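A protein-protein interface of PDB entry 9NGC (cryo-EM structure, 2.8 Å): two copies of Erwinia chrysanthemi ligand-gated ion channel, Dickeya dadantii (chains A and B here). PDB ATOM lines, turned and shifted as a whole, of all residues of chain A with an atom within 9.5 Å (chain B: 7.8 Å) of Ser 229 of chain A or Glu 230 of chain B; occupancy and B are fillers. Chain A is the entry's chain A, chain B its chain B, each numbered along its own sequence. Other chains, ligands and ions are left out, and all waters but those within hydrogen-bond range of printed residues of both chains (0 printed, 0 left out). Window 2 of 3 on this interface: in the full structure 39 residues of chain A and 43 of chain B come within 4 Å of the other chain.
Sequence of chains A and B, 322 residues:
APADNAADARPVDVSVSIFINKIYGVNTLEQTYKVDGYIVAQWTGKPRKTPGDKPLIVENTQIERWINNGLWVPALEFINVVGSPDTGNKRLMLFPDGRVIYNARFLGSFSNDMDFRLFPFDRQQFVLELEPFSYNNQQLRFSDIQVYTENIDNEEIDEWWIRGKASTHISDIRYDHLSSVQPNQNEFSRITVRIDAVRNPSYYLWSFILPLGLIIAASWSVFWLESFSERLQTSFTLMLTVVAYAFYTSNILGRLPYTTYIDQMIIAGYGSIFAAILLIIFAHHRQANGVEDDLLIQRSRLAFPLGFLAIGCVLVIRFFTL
Ser 229 of chain A touches just one residue of chain B: Glu 230 (2.2 Å). No residue of chain A comes within 4 Å of Ser 227 of chain B. No residue of chain A comes within 4 Å of Ser 229 of chain B. Of the printed residues of chain B, His 284 of chain A touches Glu 226. Of the printed residues of chain B, Gln 233 of chain A touches Gln 233 (3.3 Å). Of the printed residues of chain A, Leu 225 of chain B touches Phe 228 and Leu 232. Of the printed residues of chain B, Phe 228 of chain A touches Leu 225 (3.6 Å) and Glu 230 (3.2 Å). Thr 237 of chain A touches none of the printed residues of chain B. The nearest residue of chain A that does not touch Glu 230 of chain B is Leu 232 of chain A (4.5 Å). The nearest printed residue of chain B that does not touch Gln 287 of chain A is Trp 224 of chain B (8.6 Å).
Phe 228 of chain A touches Leu 225 of chain B, but with the chains exchanged Leu 225 of chain A does not touch Phe 228 of chain B (18.8 Å). Phe 228 of chain A touches Glu 230 of chain B, but with the chains exchanged Glu 230 of chain A does not touch Phe 228 of chain B (13.2 Å). Leu 232 of chain A touches Leu 225 of chain B, but with the chains exchanged Leu 225 of chain A does not touch Leu 232 of chain B (18.5 Å). Gln 233 of chain B touches its own counterpart, Gln 233 of chain A. 14 positions are printed for both chains.
The backbone carbonyl oxygen of Gln 233 of chain A lies within hydrogen-bond range of the side-chain hydroxyl of Thr 237 of chain A, 2.7 Å away. ND1 of His 284 of chain A lies within hydrogen-bond range of OE1 of Gln 287 of chain A, at 3.0 Å. OE1 of Glu 230 of chain B lies within hydrogen-bond range of OG of Ser 227 of chain B (3.0 Å).
Hydrophobic or aromatic side chains of chain A that line the printed part of chain B: Phe 228, Leu 232 and His 284. Along chain A the printed residues that touch a printed residue of chain B span positions 228 to 287. Printed residues of chain B that touch a printed residue of chain A: Leu 225, Glu 226, Glu 230 and Gln 233.
CZ of Phe 228 of chain A touches CD2 of Leu 225 of chain B, at 3.6 Å. Phe 228 of chain A touches Glu 230 of chain B (CE2 to OE1, 3.2 Å). CD2 of Leu 232 of chain A touches CD1 of Leu 225 of chain B, at 3.8 Å. OE2 of Glu 226 of chain B touches O of Gln 287 of chain A, at 3.7 Å.
OE1 of Gln 233 of chain A sits at hydrogen-bond distance from NE2 of Gln 233 of chain B (3.3 Å). A ring nitrogen (NE2) of His 284 of chain A lies within hydrogen-bond range of the side-chain carboxylate (OE1) of Glu 226 of chain B (2.8 Å). The side-chain carboxylate of Glu 230 of chain B sits close to the side-chain hydroxyl of Ser 229 of chain A, at 2.2 Å.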
ATOM      1  N   VAL A 222       1.740  19.368  -0.936  1.00  0.00           N
ATOM      2  CA  VAL A 222       3.007  20.042  -1.208  1.00  0.00           C
ATOM      3  C   VAL A 222       2.807  21.551  -1.382  1.00  0.00           C
ATOM      4  O   VAL A 222       3.749  22.326  -1.184  1.00  0.00           O
ATOM      5  CB  VAL A 222       3.690  19.416  -2.445  1.00  0.00           C
ATOM      6  CG1 VAL A 222       2.883  19.656  -3.702  1.00  0.00           C
ATOM      7  CG2 VAL A 222       5.125  19.879  -2.605  1.00  0.00           C
ATOM      8  N   LEU A 225       3.930  24.150   1.484  1.00  0.00           N
ATOM      9  CA  LEU A 225       5.319  24.432   1.810  1.00  0.00           C
ATOM     10  C   LEU A 225       5.671  25.872   1.454  1.00  0.00           C
ATOM     11  O   LEU A 225       5.074  26.482   0.564  1.00  0.00           O
ATOM     12  CB  LEU A 225       6.243  23.461   1.077  1.00  0.00           C
ATOM     13  CG  LEU A 225       5.926  21.980   1.301  1.00  0.00           C
ATOM     14  CD1 LEU A 225       6.878  21.095   0.519  1.00  0.00           C
ATOM     15  CD2 LEU A 225       5.964  21.637   2.779  1.00  0.00           C
ATOM     16  N   GLU A 226       6.656  26.417   2.165  1.00  0.00           N
ATOM     17  CA  GLU A 226       7.002  27.829   2.069  1.00  0.00           C
ATOM     18  C   GLU A 226       8.234  28.094   1.212  1.00  0.00           C
ATOM     19  O   GLU A 226       8.691  29.239   1.147  1.00  0.00           O
ATOM     20  CB  GLU A 226       7.213  28.409   3.469  1.00  0.00           C
ATOM     21  CG  GLU A 226       5.950  28.472   4.312  1.00  0.00           C
ATOM     22  CD  GLU A 226       6.239  28.743   5.775  1.00  0.00           C
ATOM     23  OE1 GLU A 226       7.408  28.593   6.187  1.00  0.00           O
ATOM     24  OE2 GLU A 226       5.298  29.107   6.510  1.00  0.00           O
ATOM     25  N   SER A 227       8.782  27.077   0.554  1.00  0.00           N
ATOM     26  CA  SER A 227       9.962  27.246  -0.279  1.00  0.00           C
ATOM     27  C   SER A 227       9.734  26.605  -1.640  1.00  0.00           C
ATOM     28  O   SER A 227       8.998  25.623  -1.768  1.00  0.00           O
ATOM     29  CB  SER A 227      11.210  26.652   0.384  1.00  0.00           C
ATOM     30  OG  SER A 227      11.052  25.266   0.610  1.00  0.00           O
ATOM     31  N   PHE A 228      10.377  27.179  -2.659  1.00  0.00           N
ATOM     32  CA  PHE A 228      10.138  26.741  -4.031  1.00  0.00           C
ATOM     33  C   PHE A 228      10.816  25.407  -4.324  1.00  0.00           C
ATOM     34  O   PHE A 228      10.267  24.577  -5.058  1.00  0.00           O
ATOM     35  CB  PHE A 228      10.616  27.815  -5.008  1.00  0.00           C
ATOM     36  CG  PHE A 228      10.550  27.396  -6.447  1.00  0.00           C
ATOM     37  CD1 PHE A 228       9.329  27.181  -7.064  1.00  0.00           C
ATOM     38  CD2 PHE A 228      11.709  27.224  -7.186  1.00  0.00           C
ATOM     39  CE1 PHE A 228       9.266  26.796  -8.387  1.00  0.00           C
ATOM     40  CE2 PHE A 228      11.651  26.841  -8.511  1.00  0.00           C
ATOM     41  CZ  PHE A 228      10.427  26.627  -9.112  1.00  0.00           C
ATOM     42  N   SER A 229      12.014  25.187  -3.773  1.00  0.00           N
ATOM     43  CA  SER A 229      12.742  23.949  -4.043  1.00  0.00           C
ATOM     44  C   SER A 229      12.035  22.739  -3.444  1.00  0.00           C
ATOM     45  O   SER A 229      11.962  21.679  -4.080  1.00  0.00           O
ATOM     46  CB  SER A 229      14.169  24.057  -3.509  1.00  0.00           C
ATOM     47  OG  SER A 229      14.894  25.061  -4.196  1.00  0.00           O
ATOM     48  N   GLU A 230      11.518  22.876  -2.220  1.00  0.00           N
ATOM     49  CA  GLU A 230      10.749  21.798  -1.609  1.00  0.00           C
ATOM     50  C   GLU A 230       9.443  21.553  -2.350  1.00  0.00           C
ATOM     51  O   GLU A 230       9.018  20.401  -2.485  1.00  0.00           O
ATOM     52  CB  GLU A 230      10.464  22.110  -0.141  1.00  0.00           C
ATOM     53  CG  GLU A 230      11.681  22.060   0.757  1.00  0.00           C
ATOM     54  CD  GLU A 230      11.372  22.524   2.164  1.00  0.00           C
ATOM     55  OE1 GLU A 230      10.260  23.047   2.385  1.00  0.00           O
ATOM     56  OE2 GLU A 230      12.238  22.367   3.049  1.00  0.00           O
ATOM     57  N   ARG A 231       8.794  22.616  -2.828  1.00  0.00           N
ATOM     58  CA  ARG A 231       7.589  22.448  -3.628  1.00  0.00           C
ATOM     59  C   ARG A 231       7.877  21.813  -4.977  1.00  0.00           C
ATOM     60  O   ARG A 231       6.987  21.181  -5.548  1.00  0.00           O
ATOM     61  CB  ARG A 231       6.893  23.791  -3.843  1.00  0.00           C
ATOM     62  CG  ARG A 231       6.042  24.251  -2.683  1.00  0.00           C
ATOM     63  CD  ARG A 231       5.220  25.465  -3.067  1.00  0.00           C
ATOM     64  NE  ARG A 231       6.066  26.598  -3.419  1.00  0.00           N
ATOM     65  CZ  ARG A 231       5.613  27.757  -3.875  1.00  0.00           C
ATOM     66  NH1 ARG A 231       4.319  27.980  -4.034  1.00  0.00           N
ATOM     67  NH2 ARG A 231       6.481  28.718  -4.180  1.00  0.00           N
ATOM     68  N   LEU A 232       9.097  21.956  -5.493  1.00  0.00           N
ATOM     69  CA  LEU A 232       9.407  21.491  -6.837  1.00  0.00           C
ATOM     70  C   LEU A 232       9.917  20.053  -6.864  1.00  0.00           C
ATOM     71  O   LEU A 232       9.397  19.228  -7.623  1.00  0.00           O
ATOM     72  CB  LEU A 232      10.432  22.424  -7.485  1.00  0.00           C
ATOM     73  CG  LEU A 232      10.631  22.246  -8.989  1.00  0.00           C
ATOM     74  CD1 LEU A 232       9.493  22.891  -9.756  1.00  0.00           C
ATOM     75  CD2 LEU A 232      11.966  22.824  -9.411  1.00  0.00           C
ATOM     76  N   GLN A 233      10.933  19.734  -6.055  1.00  0.00           N
ATOM     77  CA  GLN A 233      11.568  18.423  -6.181  1.00  0.00           C
ATOM     78  C   GLN A 233      10.671  17.308  -5.645  1.00  0.00           C
ATOM     79  O   GLN A 233      10.640  16.209  -6.211  1.00  0.00           O
ATOM     80  CB  GLN A 233      12.937  18.412  -5.494  1.00  0.00           C
ATOM     81  CG  GLN A 233      12.940  18.599  -3.988  1.00  0.00           C
ATOM     82  CD  GLN A 233      14.340  18.632  -3.414  1.00  0.00           C
ATOM     83  OE1 GLN A 233      15.322  18.463  -4.136  1.00  0.00           O
ATOM     84  NE2 GLN A 233      14.439  18.851  -2.108  1.00  0.00           N
ATOM     85  N   THR A 234       9.907  17.580  -4.584  1.00  0.00           N
ATOM     86  CA  THR A 234       8.991  16.571  -4.062  1.00  0.00           C
ATOM     87  C   THR A 234       7.829  16.339  -5.018  1.00  0.00           C
ATOM     88  O   THR A 234       7.374  15.201  -5.188  1.00  0.00           O
ATOM     89  CB  THR A 234       8.480  16.986  -2.683  1.00  0.00           C
ATOM     90  OG1 THR A 234       7.982  18.325  -2.745  1.00  0.00           O
ATOM     91  CG2 THR A 234       9.602  16.922  -1.659  1.00  0.00           C
ATOM     92  N   SER A 235       7.345  17.405  -5.662  1.00  0.00           N
ATOM     93  CA  SER A 235       6.295  17.260  -6.665  1.00  0.00           C
ATOM     94  C   SER A 235       6.789  16.476  -7.874  1.00  0.00           C
ATOM     95  O   SER A 235       6.052  15.651  -8.424  1.00  0.00           O
ATOM     96  CB  SER A 235       5.779  18.631  -7.089  1.00  0.00           C
ATOM     97  OG  SER A 235       4.634  18.512  -7.910  1.00  0.00           O
ATOM     98  N   PHE A 236       8.034  16.716  -8.298  1.00  0.00           N
ATOM     99  CA  PHE A 236       8.606  15.931  -9.390  1.00  0.00           C
ATOM    100  C   PHE A 236       8.760  14.465  -9.005  1.00  0.00           C
ATOM    101  O   PHE A 236       8.505  13.572  -9.822  1.00  0.00           O
ATOM    102  CB  PHE A 236       9.953  16.513  -9.814  1.00  0.00           C
ATOM    103  CG  PHE A 236       9.874  17.415 -11.009  1.00  0.00           C
ATOM    104  CD1 PHE A 236       9.705  16.887 -12.277  1.00  0.00           C
ATOM    105  CD2 PHE A 236       9.981  18.786 -10.867  1.00  0.00           C
ATOM    106  CE1 PHE A 236       9.634  17.710 -13.380  1.00  0.00           C
ATOM    107  CE2 PHE A 236       9.914  19.615 -11.968  1.00  0.00           C
ATOM    108  CZ  PHE A 236       9.739  19.076 -13.225  1.00  0.00           C
ATOM    109  N   THR A 237       9.178  14.201  -7.762  1.00  0.00           N
ATOM    110  CA  THR A 237       9.305  12.824  -7.290  1.00  0.00           C
ATOM    111  C   THR A 237       7.960  12.110  -7.277  1.00  0.00           C
ATOM    112  O   THR A 237       7.854  10.959  -7.719  1.00  0.00           O
ATOM    113  CB  THR A 237       9.930  12.805  -5.895  1.00  0.00           C
ATOM    114  OG1 THR A 237      11.115  13.608  -5.891  1.00  0.00           O
ATOM    115  CG2 THR A 237      10.284  11.389  -5.488  1.00  0.00           C
ATOM    116  N   ILE A 280       3.359  26.078  -9.989  1.00  0.00           N
ATOM    117  CA  ILE A 280       4.398  26.599  -9.103  1.00  0.00           C
ATOM    118  C   ILE A 280       5.551  27.200  -9.905  1.00  0.00           C
ATOM    119  O   ILE A 280       6.158  28.189  -9.472  1.00  0.00           O
ATOM    120  CB  ILE A 280       4.881  25.527  -8.103  1.00  0.00           C
ATOM    121  CG1 ILE A 280       5.514  24.333  -8.807  1.00  0.00           C
ATOM    122  CG2 ILE A 280       3.735  25.062  -7.223  1.00  0.00           C
ATOM    123  CD1 ILE A 280       6.199  23.382  -7.878  1.00  0.00           C
ATOM    124  N   ILE A 281       5.854  26.654 -11.089  1.00  0.00           N
ATOM    125  CA  ILE A 281       6.887  27.250 -11.936  1.00  0.00           C
ATOM    126  C   ILE A 281       6.439  28.617 -12.444  1.00  0.00           C
ATOM    127  O   ILE A 281       7.226  29.571 -12.473  1.00  0.00           O
ATOM    128  CB  ILE A 281       7.250  26.292 -13.088  1.00  0.00           C
ATOM    129  CG1 ILE A 281       8.130  25.153 -12.574  1.00  0.00           C
ATOM    130  CG2 ILE A 281       7.980  27.014 -14.210  1.00  0.00           C
ATOM    131  CD1 ILE A 281       8.436  24.109 -13.620  1.00  0.00           C
ATOM    132  N   HIS A 284       6.707  31.065  -9.554  1.00  0.00           N
ATOM    133  CA  HIS A 284       8.098  31.474  -9.380  1.00  0.00           C
ATOM    134  C   HIS A 284       8.558  32.420 -10.482  1.00  0.00           C
ATOM    135  O   HIS A 284       9.345  33.337 -10.218  1.00  0.00           O
ATOM    136  CB  HIS A 284       9.006  30.247  -9.335  1.00  0.00           C
ATOM    137  CG  HIS A 284      10.432  30.565  -9.010  1.00  0.00           C
ATOM    138  ND1 HIS A 284      10.850  30.905  -7.741  1.00  0.00           N
ATOM    139  CD2 HIS A 284      11.539  30.595  -9.790  1.00  0.00           C
ATOM    140  CE1 HIS A 284      12.151  31.129  -7.754  1.00  0.00           C
ATOM    141  NE2 HIS A 284      12.593  30.947  -8.986  1.00  0.00           N
ATOM    142  N   GLN A 287       7.702  36.038  -9.995  1.00  0.00           N
ATOM    143  CA  GLN A 287       8.574  36.748  -9.060  1.00  0.00           C
ATOM    144  C   GLN A 287       9.698  37.393  -9.867  1.00  0.00           C
ATOM    145  O   GLN A 287      10.806  36.864  -9.997  1.00  0.00           O
ATOM    146  CB  GLN A 287       9.118  35.799  -8.000  1.00  0.00           C
ATOM    147  CG  GLN A 287       8.054  35.157  -7.127  1.00  0.00           C
ATOM    148  CD  GLN A 287       8.564  33.935  -6.385  1.00  0.00           C
ATOM    149  OE1 GLN A 287       9.649  33.427  -6.673  1.00  0.00           O
ATOM    150  NE2 GLN A 287       7.782  33.456  -5.425  1.00  0.00           N
ATOM    151  N   VAL B 222      12.301  23.050 -17.435  1.00  0.00           N
ATOM    152  CA  VAL B 222      13.331  23.247 -16.417  1.00  0.00           C
ATOM    153  C   VAL B 222      14.193  24.474 -16.730  1.00  0.00           C
ATOM    154  O   VAL B 222      14.797  25.053 -15.820  1.00  0.00           O
ATOM    155  CB  VAL B 222      14.193  21.972 -16.275  1.00  0.00           C
ATOM    156  CG1 VAL B 222      14.986  21.700 -17.534  1.00  0.00           C
ATOM    157  CG2 VAL B 222      15.086  22.016 -15.050  1.00  0.00           C
ATOM    158  N   PHE B 223      14.223  24.922 -17.989  1.00  0.00           N
ATOM    159  CA  PHE B 223      15.030  26.077 -18.374  1.00  0.00           C
ATOM    160  C   PHE B 223      14.541  27.380 -17.756  1.00  0.00           C
ATOM    161  O   PHE B 223      15.298  28.354 -17.717  1.00  0.00           O
ATOM    162  CB  PHE B 223      15.044  26.228 -19.896  1.00  0.00           C
ATOM    163  CG  PHE B 223      16.109  25.423 -20.578  1.00  0.00           C
ATOM    164  CD1 PHE B 223      17.424  25.858 -20.586  1.00  0.00           C
ATOM    165  CD2 PHE B 223      15.793  24.241 -21.224  1.00  0.00           C
ATOM    166  CE1 PHE B 223      18.405  25.123 -21.216  1.00  0.00           C
ATOM    167  CE2 PHE B 223      16.771  23.502 -21.856  1.00  0.00           C
ATOM    168  CZ  PHE B 223      18.079  23.945 -21.852  1.00  0.00           C
ATOM    169  N   TRP B 224      13.299  27.423 -17.280  1.00  0.00           N
ATOM    170  CA  TRP B 224      12.736  28.642 -16.717  1.00  0.00           C
ATOM    171  C   TRP B 224      13.120  28.855 -15.258  1.00  0.00           C
ATOM    172  O   TRP B 224      12.788  29.905 -14.697  1.00  0.00           O
ATOM    173  CB  TRP B 224      11.213  28.611 -16.845  1.00  0.00           C
ATOM    174  CG  TRP B 224      10.719  28.635 -18.260  1.00  0.00           C
ATOM    175  CD1 TRP B 224      10.292  27.566 -18.991  1.00  0.00           C
ATOM    176  CD2 TRP B 224      10.600  29.779 -19.117  1.00  0.00           C
ATOM    177  NE1 TRP B 224       9.916  27.970 -20.247  1.00  0.00           N
ATOM    178  CE2 TRP B 224      10.095  29.325 -20.351  1.00  0.00           C
ATOM    179  CE3 TRP B 224      10.874  31.142 -18.961  1.00  0.00           C
ATOM    180  CZ2 TRP B 224       9.854  30.182 -21.420  1.00  0.00           C
ATOM    181  CZ3 TRP B 224      10.632  31.992 -20.024  1.00  0.00           C
ATOM    182  CH2 TRP B 224      10.131  31.508 -21.237  1.00  0.00           C
ATOM    183  N   LEU B 225      13.793  27.893 -14.635  1.00  0.00           N
ATOM    184  CA  LEU B 225      14.202  28.034 -13.246  1.00  0.00           C
ATOM    185  C   LEU B 225      15.368  29.010 -13.126  1.00  0.00           C
ATOM    186  O   LEU B 225      16.154  29.193 -14.059  1.00  0.00           O
ATOM    187  CB  LEU B 225      14.582  26.673 -12.666  1.00  0.00           C
ATOM    188  CG  LEU B 225      13.509  25.591 -12.805  1.00  0.00           C
ATOM    189  CD1 LEU B 225      13.983  24.274 -12.222  1.00  0.00           C
ATOM    190  CD2 LEU B 225      12.210  26.031 -12.153  1.00  0.00           C
ATOM    191  N   GLU B 226      15.474  29.640 -11.959  1.00  0.00           N
ATOM    192  CA  GLU B 226      16.423  30.723 -11.738  1.00  0.00           C
ATOM    193  C   GLU B 226      17.669  30.288 -10.974  1.00  0.00           C
ATOM    194  O   GLU B 226      18.494  31.139 -10.630  1.00  0.00           O
ATOM    195  CB  GLU B 226      15.738  31.872 -10.995  1.00  0.00           C
ATOM    196  CG  GLU B 226      14.667  32.582 -11.806  1.00  0.00           C
ATOM    197  CD  GLU B 226      13.799  33.488 -10.955  1.00  0.00           C
ATOM    198  OE1 GLU B 226      13.830  33.347  -9.715  1.00  0.00           O
ATOM    199  OE2 GLU B 226      13.087  34.338 -11.526  1.00  0.00           O
ATOM    200  N   SER B 227      17.832  28.996 -10.704  1.00  0.00           N
ATOM    201  CA  SER B 227      18.989  28.503  -9.975  1.00  0.00           C
ATOM    202  C   SER B 227      19.606  27.324 -10.714  1.00  0.00           C
ATOM    203  O   SER B 227      18.913  26.567 -11.400  1.00  0.00           O
ATOM    204  CB  SER B 227      18.622  28.096  -8.543  1.00  0.00           C
ATOM    205  OG  SER B 227      17.656  27.066  -8.541  1.00  0.00           O
ATOM    206  N   PHE B 228      20.924  27.180 -10.567  1.00  0.00           N
ATOM    207  CA  PHE B 228      21.653  26.170 -11.328  1.00  0.00           C
ATOM    208  C   PHE B 228      21.416  24.768 -10.778  1.00  0.00           C
ATOM    209  O   PHE B 228      21.335  23.803 -11.547  1.00  0.00           O
ATOM    210  CB  PHE B 228      23.145  26.502 -11.334  1.00  0.00           C
ATOM    211  CG  PHE B 228      23.999  25.443 -11.966  1.00  0.00           C
ATOM    212  CD1 PHE B 228      23.910  25.181 -13.322  1.00  0.00           C
ATOM    213  CD2 PHE B 228      24.895  24.711 -11.204  1.00  0.00           C
ATOM    214  CE1 PHE B 228      24.693  24.207 -13.905  1.00  0.00           C
ATOM    215  CE2 PHE B 228      25.682  23.736 -11.784  1.00  0.00           C
ATOM    216  CZ  PHE B 228      25.581  23.486 -13.137  1.00  0.00           C
ATOM    217  N   SER B 229      21.314  24.633  -9.452  1.00  0.00           N
ATOM    218  CA  SER B 229      21.130  23.314  -8.850  1.00  0.00           C
ATOM    219  C   SER B 229      19.770  22.721  -9.203  1.00  0.00           C
ATOM    220  O   SER B 229      19.666  21.520  -9.489  1.00  0.00           O
ATOM    221  CB  SER B 229      21.300  23.404  -7.335  1.00  0.00           C
ATOM    222  OG  SER B 229      22.622  23.775  -6.994  1.00  0.00           O
ATOM    223  N   GLU B 230      18.718  23.545  -9.180  1.00  0.00           N
ATOM    224  CA  GLU B 230      17.398  23.082  -9.589  1.00  0.00           C
ATOM    225  C   GLU B 230      17.357  22.750 -11.074  1.00  0.00           C
ATOM    226  O   GLU B 230      16.691  21.787 -11.471  1.00  0.00           O
ATOM    227  CB  GLU B 230      16.338  24.132  -9.262  1.00  0.00           C
ATOM    228  CG  GLU B 230      16.069  24.308  -7.783  1.00  0.00           C
ATOM    229  CD  GLU B 230      15.127  25.461  -7.508  1.00  0.00           C
ATOM    230  OE1 GLU B 230      14.830  26.223  -8.452  1.00  0.00           O
ATOM    231  OE2 GLU B 230      14.684  25.608  -6.350  1.00  0.00           O
ATOM    232  N   ARG B 231      18.050  23.532 -11.902  1.00  0.00           N
ATOM    233  CA  ARG B 231      18.132  23.218 -13.321  1.00  0.00           C
ATOM    234  C   ARG B 231      18.931  21.952 -13.584  1.00  0.00           C
ATOM    235  O   ARG B 231      18.706  21.299 -14.606  1.00  0.00           O
ATOM    236  CB  ARG B 231      18.757  24.377 -14.096  1.00  0.00           C
ATOM    237  CG  ARG B 231      17.803  25.504 -14.416  1.00  0.00           C
ATOM    238  CD  ARG B 231      18.442  26.493 -15.369  1.00  0.00           C
ATOM    239  NE  ARG B 231      19.622  27.119 -14.786  1.00  0.00           N
ATOM    240  CZ  ARG B 231      20.421  27.956 -15.430  1.00  0.00           C
ATOM    241  NH1 ARG B 231      20.190  28.308 -16.683  1.00  0.00           N
ATOM    242  NH2 ARG B 231      21.482  28.454 -14.801  1.00  0.00           N
ATOM    243  N   LEU B 232      19.847  21.588 -12.689  1.00  0.00           N
ATOM    244  CA  LEU B 232      20.741  20.466 -12.938  1.00  0.00           C
ATOM    245  C   LEU B 232      20.182  19.140 -12.427  1.00  0.00           C
ATOM    246  O   LEU B 232      20.135  18.160 -13.180  1.00  0.00           O
ATOM    247  CB  LEU B 232      22.106  20.740 -12.304  1.00  0.00           C
ATOM    248  CG  LEU B 232      23.233  19.802 -12.729  1.00  0.00           C
ATOM    249  CD1 LEU B 232      23.747  20.178 -14.106  1.00  0.00           C
ATOM    250  CD2 LEU B 232      24.350  19.829 -11.707  1.00  0.00           C
ATOM    251  N   GLN B 233      19.765  19.083 -11.157  1.00  0.00           N
ATOM    252  CA  GLN B 233      19.397  17.791 -10.579  1.00  0.00           C
ATOM    253  C   GLN B 233      18.067  17.284 -11.135  1.00  0.00           C
ATOM    254  O   GLN B 233      17.904  16.076 -11.352  1.00  0.00           O
ATOM    255  CB  GLN B 233      19.366  17.868  -9.050  1.00  0.00           C
ATOM    256  CG  GLN B 233      18.315  18.777  -8.439  1.00  0.00           C
ATOM    257  CD  GLN B 233      18.406  18.829  -6.929  1.00  0.00           C
ATOM    258  OE1 GLN B 233      19.226  18.142  -6.322  1.00  0.00           O
ATOM    259  NE2 GLN B 233      17.560  19.647  -6.313  1.00  0.00           N
ATOM    260  N   THR B 234      17.122  18.186 -11.409  1.00  0.00           N
ATOM    261  CA  THR B 234      15.853  17.765 -11.992  1.00  0.00           C
ATOM    262  C   THR B 234      16.035  17.309 -13.433  1.00  0.00           C
ATOM    263  O   THR B 234      15.395  16.346 -13.873  1.00  0.00           O
ATOM    264  CB  THR B 234      14.833  18.900 -11.910  1.00  0.00           C
ATOM    265  OG1 THR B 234      15.410  20.095 -12.442  1.00  0.00           O
ATOM    266  CG2 THR B 234      14.425  19.145 -10.467  1.00  0.00           C
ATOM    267  N   SER B 235      16.917  17.981 -14.179  1.00  0.00           N
ATOM    268  CA  SER B 235      17.223  17.554 -15.540  1.00  0.00           C
ATOM    269  C   SER B 235      17.912  16.196 -15.553  1.00  0.00           C
ATOM    270  O   SER B 235      17.624  15.361 -16.418  1.00  0.00           O
ATOM    271  CB  SER B 235      18.088  18.600 -16.237  1.00  0.00           C
ATOM    272  OG  SER B 235      18.234  18.304 -17.612  1.00  0.00           O
ATOM    273  N   PHE B 236      18.817  15.953 -14.600  1.00  0.00           N
ATOM    274  CA  PHE B 236      19.444  14.637 -14.495  1.00  0.00           C
ATOM    275  C   PHE B 236      18.426  13.560 -14.141  1.00  0.00           C
ATOM    276  O   PHE B 236      18.483  12.445 -14.672  1.00  0.00           O
ATOM    277  CB  PHE B 236      20.569  14.666 -13.462  1.00  0.00           C
ATOM    278  CG  PHE B 236      21.932  14.848 -14.057  1.00  0.00           C
ATOM    279  CD1 PHE B 236      22.560  13.800 -14.710  1.00  0.00           C
ATOM    280  CD2 PHE B 236      22.592  16.058 -13.955  1.00  0.00           C
ATOM    281  CE1 PHE B 236      23.815  13.960 -15.258  1.00  0.00           C
ATOM    282  CE2 PHE B 236      23.850  16.223 -14.498  1.00  0.00           C
ATOM    283  CZ  PHE B 236      24.460  15.173 -15.151  1.00  0.00           C
ATOM    284  N   ILE B 280      23.378  23.908 -19.919  1.00  0.00           N
ATOM    285  CA  ILE B 280      23.358  24.597 -18.629  1.00  0.00           C
ATOM    286  C   ILE B 280      24.711  24.489 -17.929  1.00  0.00           C
ATOM    287  O   ILE B 280      25.128  25.428 -17.238  1.00  0.00           O
ATOM    288  CB  ILE B 280      22.201  24.098 -17.739  1.00  0.00           C
ATOM    289  CG1 ILE B 280      22.335  22.617 -17.403  1.00  0.00           C
ATOM    290  CG2 ILE B 280      20.861  24.358 -18.406  1.00  0.00           C
ATOM    291  CD1 ILE B 280      21.370  22.147 -16.361  1.00  0.00           C
